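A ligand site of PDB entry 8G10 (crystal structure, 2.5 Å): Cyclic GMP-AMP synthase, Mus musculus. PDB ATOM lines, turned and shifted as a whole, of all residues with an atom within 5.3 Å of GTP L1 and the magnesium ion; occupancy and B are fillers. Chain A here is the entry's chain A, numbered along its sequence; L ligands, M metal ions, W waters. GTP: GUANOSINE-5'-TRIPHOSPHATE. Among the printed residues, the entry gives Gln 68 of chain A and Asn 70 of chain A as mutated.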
ATOM      1  N   THR A  54     -26.133  34.545  -8.582  1.00  0.00           N
ATOM      2  CA  THR A  54     -25.646  33.964  -7.324  1.00  0.00           C
ATOM      3  C   THR A  54     -24.548  32.927  -7.597  1.00  0.00           C
ATOM      4  O   THR A  54     -24.146  32.696  -8.743  1.00  0.00           O
ATOM      5  CB  THR A  54     -26.792  33.313  -6.529  1.00  0.00           C
ATOM      6  OG1 THR A  54     -27.485  32.400  -7.388  1.00  0.00           O
ATOM      7  CG2 THR A  54     -27.764  34.356  -6.055  1.00  0.00           C
ATOM      8  N   GLY A  55     -24.053  32.292  -6.521  1.00  0.00           N
ATOM      9  CA  GLY A  55     -23.065  31.234  -6.647  1.00  0.00           C
ATOM     10  C   GLY A  55     -21.666  31.774  -6.909  1.00  0.00           C
ATOM     11  O   GLY A  55     -21.417  32.983  -6.939  1.00  0.00           O
ATOM     12  N   SER A  56     -20.757  30.837  -7.174  1.00  0.00           N
ATOM     13  CA  SER A  56     -19.334  31.119  -7.029  1.00  0.00           C
ATOM     14  C   SER A  56     -18.865  32.202  -7.997  1.00  0.00           C
ATOM     15  O   SER A  56     -18.025  33.035  -7.643  1.00  0.00           O
ATOM     16  CB  SER A  56     -18.502  29.833  -7.213  1.00  0.00           C
ATOM     17  OG  SER A  56     -18.752  29.183  -8.455  1.00  0.00           O
ATOM     18  N   GLN A  68     -19.540  27.440 -15.108  1.00  0.00           N
ATOM     19  CA  GLN A  68     -20.777  27.138 -14.395  1.00  0.00           C
ATOM     20  C   GLN A  68     -21.328  28.412 -13.750  1.00  0.00           C
ATOM     21  O   GLN A  68     -20.688  28.976 -12.865  1.00  0.00           O
ATOM     22  CB  GLN A  68     -20.553  26.058 -13.344  1.00  0.00           C
ATOM     23  CG  GLN A  68     -21.796  25.233 -13.080  1.00  0.00           C
ATOM     24  CD  GLN A  68     -22.585  25.793 -11.934  1.00  0.00           C
ATOM     25  OE1 GLN A  68     -22.226  26.827 -11.362  1.00  0.00           O
ATOM     26  NE2 GLN A  68     -23.654  25.100 -11.561  1.00  0.00           N
ATOM     27  N   PHE A  69     -22.525  28.822 -14.173  1.00  0.00           N
ATOM     28  CA  PHE A  69     -23.175  30.038 -13.731  1.00  0.00           C
ATOM     29  C   PHE A  69     -24.474  29.712 -13.005  1.00  0.00           C
ATOM     30  O   PHE A  69     -25.195  28.776 -13.373  1.00  0.00           O
ATOM     31  CB  PHE A  69     -23.482  30.965 -14.912  1.00  0.00           C
ATOM     32  CG  PHE A  69     -22.251  31.480 -15.620  1.00  0.00           C
ATOM     33  CD1 PHE A  69     -21.506  30.657 -16.442  1.00  0.00           C
ATOM     34  CD2 PHE A  69     -21.820  32.784 -15.431  1.00  0.00           C
ATOM     35  CE1 PHE A  69     -20.380  31.111 -17.079  1.00  0.00           C
ATOM     36  CE2 PHE A  69     -20.689  33.256 -16.053  1.00  0.00           C
ATOM     37  CZ  PHE A  69     -19.969  32.420 -16.877  1.00  0.00           C
ATOM     38  N   ASN A  70     -24.788  30.495 -11.986  1.00  0.00           N
ATOM     39  CA  ASN A  70     -25.987  30.285 -11.189  1.00  0.00           C
ATOM     40  C   ASN A  70     -26.829  31.545 -11.228  1.00  0.00           C
ATOM     41  O   ASN A  70     -26.337  32.640 -10.900  1.00  0.00           O
ATOM     42  CB  ASN A  70     -25.632  29.903  -9.753  1.00  0.00           C
ATOM     43  CG  ASN A  70     -24.835  28.616  -9.690  1.00  0.00           C
ATOM     44  OD1 ASN A  70     -23.600  28.646  -9.562  1.00  0.00           O
ATOM     45  ND2 ASN A  70     -25.520  27.477  -9.803  1.00  0.00           N
ATOM     46  N   VAL A  71     -28.089  31.423 -11.633  1.00  0.00           N
ATOM     47  CA  VAL A  71     -28.953  32.605 -11.680  1.00  0.00           C
ATOM     48  C   VAL A  71     -30.335  32.227 -11.182  1.00  0.00           C
ATOM     49  O   VAL A  71     -30.900  31.216 -11.592  1.00  0.00           O
ATOM     50  CB  VAL A  71     -28.982  33.233 -13.094  1.00  0.00           C
ATOM     51  CG1 VAL A  71     -29.240  32.198 -14.131  1.00  0.00           C
ATOM     52  CG2 VAL A  71     -30.026  34.307 -13.178  1.00  0.00           C
ATOM     53  N   MET A  72     -30.873  33.029 -10.258  1.00  0.00           N
ATOM     54  CA  MET A  72     -32.212  32.843  -9.744  1.00  0.00           C
ATOM     55  C   MET A  72     -33.199  33.750 -10.486  1.00  0.00           C
ATOM     56  O   MET A  72     -32.943  34.943 -10.646  1.00  0.00           O
ATOM     57  CB  MET A  72     -32.265  33.111  -8.244  1.00  0.00           C
ATOM     58  CG  MET A  72     -31.234  32.296  -7.467  1.00  0.00           C
ATOM     59  SD  MET A  72     -31.280  32.418  -5.648  1.00  0.00           S
ATOM     60  CE  MET A  72     -33.031  32.557  -5.327  1.00  0.00           C
ATOM     61  N   LYS A 145     -32.978  16.191 -13.389  1.00  0.00           N
ATOM     62  CA  LYS A 145     -32.714  15.346 -12.208  1.00  0.00           C
ATOM     63  C   LYS A 145     -33.924  15.318 -11.296  1.00  0.00           C
ATOM     64  O   LYS A 145     -34.386  16.394 -10.874  1.00  0.00           O
ATOM     65  CB  LYS A 145     -31.531  15.889 -11.428  1.00  0.00           C
ATOM     66  CG  LYS A 145     -30.187  15.565 -11.986  1.00  0.00           C
ATOM     67  CD  LYS A 145     -29.165  15.555 -10.850  1.00  0.00           C
ATOM     68  CE  LYS A 145     -29.835  15.401  -9.466  1.00  0.00           C
ATOM     69  NZ  LYS A 145     -28.849  15.233  -8.366  1.00  0.00           N
ATOM     70  N   GLY A 147     -36.059  15.511  -8.057  1.00  0.00           N
ATOM     71  CA  GLY A 147     -35.758  16.287  -6.853  1.00  0.00           C
ATOM     72  C   GLY A 147     -34.648  17.315  -7.010  1.00  0.00           C
ATOM     73  O   GLY A 147     -33.796  17.435  -6.115  1.00  0.00           O
ATOM     74  N   SER A 148     -34.611  18.041  -8.118  1.00  0.00           N
ATOM     75  CA  SER A 148     -33.616  19.098  -8.311  1.00  0.00           C
ATOM     76  C   SER A 148     -34.326  20.396  -8.697  1.00  0.00           C
ATOM     77  O   SER A 148     -35.180  20.390  -9.608  1.00  0.00           O
ATOM     78  CB  SER A 148     -32.581  18.724  -9.365  1.00  0.00           C
ATOM     79  OG  SER A 148     -31.697  19.800  -9.587  1.00  0.00           O
ATOM     80  N   PRO A 149     -34.007  21.507  -8.054  1.00  0.00           N
ATOM     81  CA  PRO A 149     -34.755  22.745  -8.323  1.00  0.00           C
ATOM     82  C   PRO A 149     -34.400  23.402  -9.650  1.00  0.00           C
ATOM     83  O   PRO A 149     -35.078  24.372 -10.024  1.00  0.00           O
ATOM     84  CB  PRO A 149     -34.366  23.634  -7.145  1.00  0.00           C
ATOM     85  CG  PRO A 149     -32.977  23.192  -6.844  1.00  0.00           C
ATOM     86  CD  PRO A 149     -32.960  21.705  -7.041  1.00  0.00           C
ATOM     87  N   ALA A 150     -33.397  22.922 -10.367  1.00  0.00           N
ATOM     88  CA  ALA A 150     -32.763  23.708 -11.427  1.00  0.00           C
ATOM     89  C   ALA A 150     -33.269  23.318 -12.807  1.00  0.00           C
ATOM     90  O   ALA A 150     -33.725  22.198 -13.047  1.00  0.00           O
ATOM     91  CB  ALA A 150     -31.245  23.566 -11.383  1.00  0.00           C
ATOM     92  N   ASP A 164     -27.388  26.930 -14.320  1.00  0.00           N
ATOM     93  CA  ASP A 164     -28.508  26.470 -13.504  1.00  0.00           C
ATOM     94  C   ASP A 164     -29.465  27.637 -13.295  1.00  0.00           C
ATOM     95  O   ASP A 164     -29.148  28.575 -12.556  1.00  0.00           O
ATOM     96  CB  ASP A 164     -28.004  25.959 -12.155  1.00  0.00           C
ATOM     97  CG  ASP A 164     -27.275  24.623 -12.248  1.00  0.00           C
ATOM     98  OD1 ASP A 164     -27.291  23.979 -13.328  1.00  0.00           O
ATOM     99  OD2 ASP A 164     -26.695  24.189 -11.221  1.00  0.00           O
ATOM    100  N   ILE A 166     -32.626  28.741 -11.454  1.00  0.00           N
ATOM    101  CA  ILE A 166     -33.378  28.283 -10.289  1.00  0.00           C
ATOM    102  C   ILE A 166     -34.616  29.157 -10.153  1.00  0.00           C
ATOM    103  O   ILE A 166     -34.514  30.380  -9.946  1.00  0.00           O
ATOM    104  CB  ILE A 166     -32.515  28.303  -9.027  1.00  0.00           C
ATOM    105  CG1 ILE A 166     -31.116  27.763  -9.363  1.00  0.00           C
ATOM    106  CG2 ILE A 166     -33.133  27.486  -7.963  1.00  0.00           C
ATOM    107  N   VAL A 205     -37.086  27.480  -2.967  1.00  0.00           N
ATOM    108  CA  VAL A 205     -36.822  26.853  -4.254  1.00  0.00           C
ATOM    109  C   VAL A 205     -37.465  25.468  -4.250  1.00  0.00           C
ATOM    110  O   VAL A 205     -37.611  24.865  -3.177  1.00  0.00           O
ATOM    111  CB  VAL A 205     -35.314  26.771  -4.534  1.00  0.00           C
ATOM    112  CG1 VAL A 205     -34.715  28.175  -4.520  1.00  0.00           C
ATOM    113  CG2 VAL A 205     -34.622  25.851  -3.542  1.00  0.00           C
ATOM    114  N   ARG A 221     -37.700  24.375  -0.506  1.00  0.00           N
ATOM    115  CA  ARG A 221     -36.519  24.488   0.342  1.00  0.00           C
ATOM    116  C   ARG A 221     -36.058  25.941   0.439  1.00  0.00           C
ATOM    117  O   ARG A 221     -36.038  26.662  -0.568  1.00  0.00           O
ATOM    118  CB  ARG A 221     -35.364  23.630  -0.189  1.00  0.00           C
ATOM    119  CG  ARG A 221     -34.170  23.604   0.764  1.00  0.00           C
ATOM    120  CD  ARG A 221     -33.030  22.758   0.243  1.00  0.00           C
ATOM    121  NE  ARG A 221     -32.411  23.350  -0.936  1.00  0.00           N
ATOM    122  CZ  ARG A 221     -31.527  22.708  -1.688  1.00  0.00           C
ATOM    123  NH1 ARG A 221     -31.146  21.480  -1.406  1.00  0.00           N
ATOM    124  NH2 ARG A 221     -31.009  23.317  -2.757  1.00  0.00           N
ATOM    125  N   LEU A 222     -35.681  26.371   1.636  1.00  0.00           N
ATOM    126  CA  LEU A 222     -35.187  27.721   1.836  1.00  0.00           C
ATOM    127  C   LEU A 222     -33.876  27.934   1.091  1.00  0.00           C
ATOM    128  O   LEU A 222     -33.001  27.070   1.075  1.00  0.00           O
ATOM    129  CB  LEU A 222     -34.971  28.013   3.317  1.00  0.00           C
ATOM    130  CG  LEU A 222     -36.230  28.306   4.109  1.00  0.00           C
ATOM    131  CD1 LEU A 222     -35.958  28.243   5.593  1.00  0.00           C
ATOM    132  CD2 LEU A 222     -36.813  29.672   3.697  1.00  0.00           C
ATOM    133  N   SER A 223     -33.730  29.111   0.493  1.00  0.00           N
ATOM    134  CA  SER A 223     -32.478  29.516  -0.115  1.00  0.00           C
ATOM    135  C   SER A 223     -31.996  30.839   0.456  1.00  0.00           C
ATOM    136  O   SER A 223     -32.782  31.772   0.637  1.00  0.00           O
ATOM    137  CB  SER A 223     -32.601  29.666  -1.615  1.00  0.00           C
ATOM    138  OG  SER A 223     -31.376  30.132  -2.121  1.00  0.00           O
ATOM    139  N   PHE A 224     -30.683  30.934   0.654  1.00  0.00           N
ATOM    140  CA  PHE A 224     -30.022  32.099   1.212  1.00  0.00           C
ATOM    141  C   PHE A 224     -28.881  32.581   0.312  1.00  0.00           C
ATOM    142  O   PHE A 224     -27.928  33.190   0.775  1.00  0.00           O
ATOM    143  CB  PHE A 224     -29.523  31.786   2.615  1.00  0.00           C
ATOM    144  CG  PHE A 224     -30.630  31.457   3.568  1.00  0.00           C
ATOM    145  CD1 PHE A 224     -31.434  32.461   4.087  1.00  0.00           C
ATOM    146  CD2 PHE A 224     -30.913  30.129   3.878  1.00  0.00           C
ATOM    147  CE1 PHE A 224     -32.470  32.157   4.938  1.00  0.00           C
ATOM    148  CE2 PHE A 224     -31.982  29.810   4.737  1.00  0.00           C
ATOM    149  CZ  PHE A 224     -32.749  30.833   5.260  1.00  0.00           C
ATOM    150  N   SER A 225     -28.976  32.292  -0.981  1.00  0.00           N
ATOM    151  CA  SER A 225     -27.908  32.629  -1.906  1.00  0.00           C
ATOM    152  C   SER A 225     -27.615  34.121  -1.931  1.00  0.00           C
ATOM    153  O   SER A 225     -26.482  34.526  -2.200  1.00  0.00           O
ATOM    154  CB  SER A 225     -28.270  32.149  -3.297  1.00  0.00           C
ATOM    155  OG  SER A 225     -28.570  30.787  -3.236  1.00  0.00           O
HETATM  156  PG  GTP L   1     -29.203  16.896  -3.769  1.00  0.00           P
HETATM  157  O1G GTP L   1     -29.212  15.389  -3.780  1.00  0.00           O
HETATM  158  O2G GTP L   1     -29.155  17.384  -2.337  1.00  0.00           O
HETATM  159  O3G GTP L   1     -30.484  17.382  -4.432  1.00  0.00           O
HETATM  160  O3B GTP L   1     -27.869  17.402  -4.567  1.00  0.00           O
HETATM  161  PB  GTP L   1     -27.962  18.117  -6.021  1.00  0.00           P
HETATM  162  O1B GTP L   1     -26.720  17.828  -6.824  1.00  0.00           O
HETATM  163  O2B GTP L   1     -29.246  17.715  -6.765  1.00  0.00           O
HETATM  164  O3A GTP L   1     -27.993  19.695  -5.696  1.00  0.00           O
HETATM  165  PA  GTP L   1     -29.338  20.502  -5.299  1.00  0.00           P
HETATM  166  O1A GTP L   1     -30.618  19.713  -5.515  1.00  0.00           O
HETATM  167  O2A GTP L   1     -29.286  21.030  -3.881  1.00  0.00           O
HETATM  168  O5' GTP L   1     -29.331  21.710  -6.370  1.00  0.00           O
HETATM  169  C5' GTP L   1     -29.030  21.491  -7.732  1.00  0.00           C
HETATM  170  C4' GTP L   1     -28.366  22.736  -8.272  1.00  0.00           C
HETATM  171  O4' GTP L   1     -29.341  23.767  -8.346  1.00  0.00           O
HETATM  172  C3' GTP L   1     -27.260  23.296  -7.384  1.00  0.00           C
HETATM  173  O3' GTP L   1     -26.003  22.741  -7.673  1.00  0.00           O
HETATM  174  C2' GTP L   1     -27.310  24.777  -7.725  1.00  0.00           C
HETATM  175  O2' GTP L   1     -26.620  24.965  -8.939  1.00  0.00           O
HETATM  176  C1' GTP L   1     -28.795  25.020  -7.958  1.00  0.00           C
HETATM  177  N9  GTP L   1     -29.353  25.454  -6.650  1.00  0.00           N
HETATM  178  C8  GTP L   1     -29.875  24.653  -5.657  1.00  0.00           C
HETATM  179  N7  GTP L   1     -30.267  25.429  -4.631  1.00  0.00           N
HETATM  180  C5  GTP L   1     -29.993  26.727  -4.936  1.00  0.00           C
HETATM  181  C6  GTP L   1     -30.188  27.939  -4.246  1.00  0.00           C
HETATM  182  O6  GTP L   1     -30.675  27.950  -3.115  1.00  0.00           O
HETATM  183  N1  GTP L   1     -29.801  29.129  -4.841  1.00  0.00           N
HETATM  184  C2  GTP L   1     -29.225  29.112  -6.095  1.00  0.00           C
HETATM  185  N2  GTP L   1     -28.839  30.242  -6.689  1.00  0.00           N
HETATM  186  N3  GTP L   1     -29.049  27.918  -6.769  1.00  0.00           N
HETATM  187  C4  GTP L   1     -29.428  26.749  -6.198  1.00  0.00           C
HETATM  188  PG  GTP L   2     -19.421  25.998  -7.602  1.00  0.00           P
HETATM  189  O1G GTP L   2     -19.188  24.527  -7.376  1.00  0.00           O
HETATM  190  O2G GTP L   2     -20.434  26.139  -8.708  1.00  0.00           O
HETATM  191  O3G GTP L   2     -18.136  26.644  -8.048  1.00  0.00           O
HETATM  192  O3B GTP L   2     -19.958  26.734  -6.248  1.00  0.00           O
HETATM  193  PB  GTP L   2     -21.457  27.339  -6.111  1.00  0.00           P
HETATM  194  O1B GTP L   2     -21.611  28.098  -4.839  1.00  0.00           O
HETATM  195  O2B GTP L   2     -21.899  28.200  -7.271  1.00  0.00           O
HETATM  196  O3A GTP L   2     -22.320  25.974  -6.018  1.00  0.00           O
HETATM  197  PA  GTP L   2     -23.582  25.571  -6.949  1.00  0.00           P
HETATM  198  O1A GTP L   2     -23.823  24.077  -6.818  1.00  0.00           O
HETATM  199  O2A GTP L   2     -23.288  25.934  -8.373  1.00  0.00           O
HETATM  200  O5' GTP L   2     -24.868  26.289  -6.315  1.00  0.00           O
HETATM  201  C5' GTP L   2     -25.072  27.691  -6.344  1.00  0.00           C
HETATM  202  C4' GTP L   2     -25.623  28.215  -5.018  1.00  0.00           C
HETATM  203  O4' GTP L   2     -26.774  27.485  -4.658  1.00  0.00           O
HETATM  204  C3' GTP L   2     -24.680  28.107  -3.810  1.00  0.00           C
HETATM  205  O3' GTP L   2     -23.800  29.209  -3.695  1.00  0.00           O
HETATM  206  C2' GTP L   2     -25.666  28.037  -2.640  1.00  0.00           C
HETATM  207  O2' GTP L   2     -26.019  29.351  -2.216  1.00  0.00           O
HETATM  208  C1' GTP L   2     -26.895  27.359  -3.240  1.00  0.00           C
HETATM  209  N9  GTP L   2     -26.942  25.922  -2.883  1.00  0.00           N
HETATM  210  C8  GTP L   2     -26.367  24.898  -3.617  1.00  0.00           C
HETATM  211  N7  GTP L   2     -26.614  23.724  -2.991  1.00  0.00           N
HETATM  212  C5  GTP L   2     -27.347  23.984  -1.881  1.00  0.00           C
HETATM  213  C6  GTP L   2     -27.878  23.153  -0.884  1.00  0.00           C
HETATM  214  O6  GTP L   2     -27.709  21.927  -0.931  1.00  0.00           O
HETATM  215  N1  GTP L   2     -28.610  23.718   0.153  1.00  0.00           N
HETATM  216  C2  GTP L   2     -28.795  25.094   0.218  1.00  0.00           C
HETATM  217  N3  GTP L   2     -28.261  25.888  -0.778  1.00  0.00           N
HETATM  218  C4  GTP L   2     -27.556  25.356  -1.799  1.00  0.00           C
HETATM  219 MG    MG M   1     -21.742  27.399  -9.225  1.00  0.00          MG
HETATM  220  O   HOH W   1     -20.810  28.867 -10.244  1.00  0.00           O
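Water W1 bridges O of Gln 68 and OG of Ser 56.
Residues that only touch GTP L1: Ile 166 (3.3 Å), Pro 149 (3.4 Å), Ala 150 (3.6 Å), Ser 148 (3.7 Å) and Gly 147 (3.7 Å). Hydrophobic or aromatic side chains within 4 Å of GTP L1: Met 72, Pro 149, Ala 150 and Ile 166. Of the 21 residues printed, 14 come within 4 Å of GTP L1. The nearest printed residue that does not touch GTP L1 is Val 205 (4.3 Å).
Merely in contact with the magnesium ion: Ser 56 (3.6 Å). Of the 21 residues printed, 3 come within 4 Å of the magnesium ion. The nearest printed residue that does not touch the magnesium ion is Gly 55 (4.8 Å).
The magnesium ion is bound by O2G of GTP L2. Water W1 binds the magnesium ion (2.0 Å). The magnesium ion is bound by an oxygen (O2B) of GTP L2 (2.1 Å). The side-chain amide oxygen (OD1) of Asn 70 is bound to the magnesium ion. The side-chain amide oxygen (OE1) of Gln 68 is bound to the magnesium ion (2.3 Å). An oxygen (O2A) of GTP L2 is bound to the magnesium ion, 2.3 Å away.
An oxygen (O1A) of GTP L2 sits at hydrogen-bond distance from an oxygen (O3') of GTP L1, at 2.7 Å.
The side-chain amide nitrogen (ND2) of Asn 70 sits at hydrogen-bond distance from an oxygen (O2') of GTP L1. OD2 of Asp 164 lies within hydrogen-bond range of O2' of GTP L1 (2.4 Å). OG of Ser 223 sits at hydrogen-bond distance from O6 of GTP L1 (2.5 Å). A nitrogen (N1) of GTP L1 lies within hydrogen-bond range of the side-chain hydroxyl (OG) of Ser 225, 2.6 Å away. A nitrogen (N2) of GTP L1 is in hydrogen-bond range of the side-chain hydroxyl (OG1) of Thr 54. The guanidinium group (NH2) of Arg 221 is in salt-bridge range of an oxygen (O2A) of GTP L1 (3.1 Å). The side-chain amino group (NZ) of Lys 145 lies within salt-bridge range of an oxygen (O2B) of GTP L1 (3.0 Å). The side-chain sulfur of Met 72 lies close to a nitrogen (N2) of GTP L1, at 3.4 Å. O2' of GTP L2 lies within hydrogen-bond range of OG of Ser 225 (3.1 Å). The guanidinium group of Arg 221 sits at hydrogen-bond distance from an oxygen (O6) of GTP L2. N of Ser 56 lies close to O2B of GTP L2, at 2.9 Å. O3G of GTP L2 sits at hydrogen-bond distance from OG of Ser 56 (2.6 Å).
The backbone NH of Thr 54 sits at hydrogen-bond distance from the backbone carbonyl oxygen of Asn 70 (3.0 Å). The side-chain amide nitrogen (NE2) of Gln 68 sits at hydrogen-bond distance from the side-chain carboxylate (OD2) of Asp 164 (3.2 Å). O of Asp 164 lies within hydrogen-bond range of N of Val 71 (3.2 Å). The backbone NH (N) of Asp 164 is in hydrogen-bond range of the backbone carbonyl oxygen (O) of Phe 69 (3.0 Å). The side-chain hydroxyl (OG) of Ser 223 lies within hydrogen-bond range of the side-chain hydroxyl (OG) of Ser 225 (3.1 Å). N of Arg 221 sits at hydrogen-bond distance from O of Val 205, 2.7 Å away. The backbone carbonyl oxygen (O) of Val 71 is in hydrogen-bond range of the backbone NH (N) of Ile 166.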
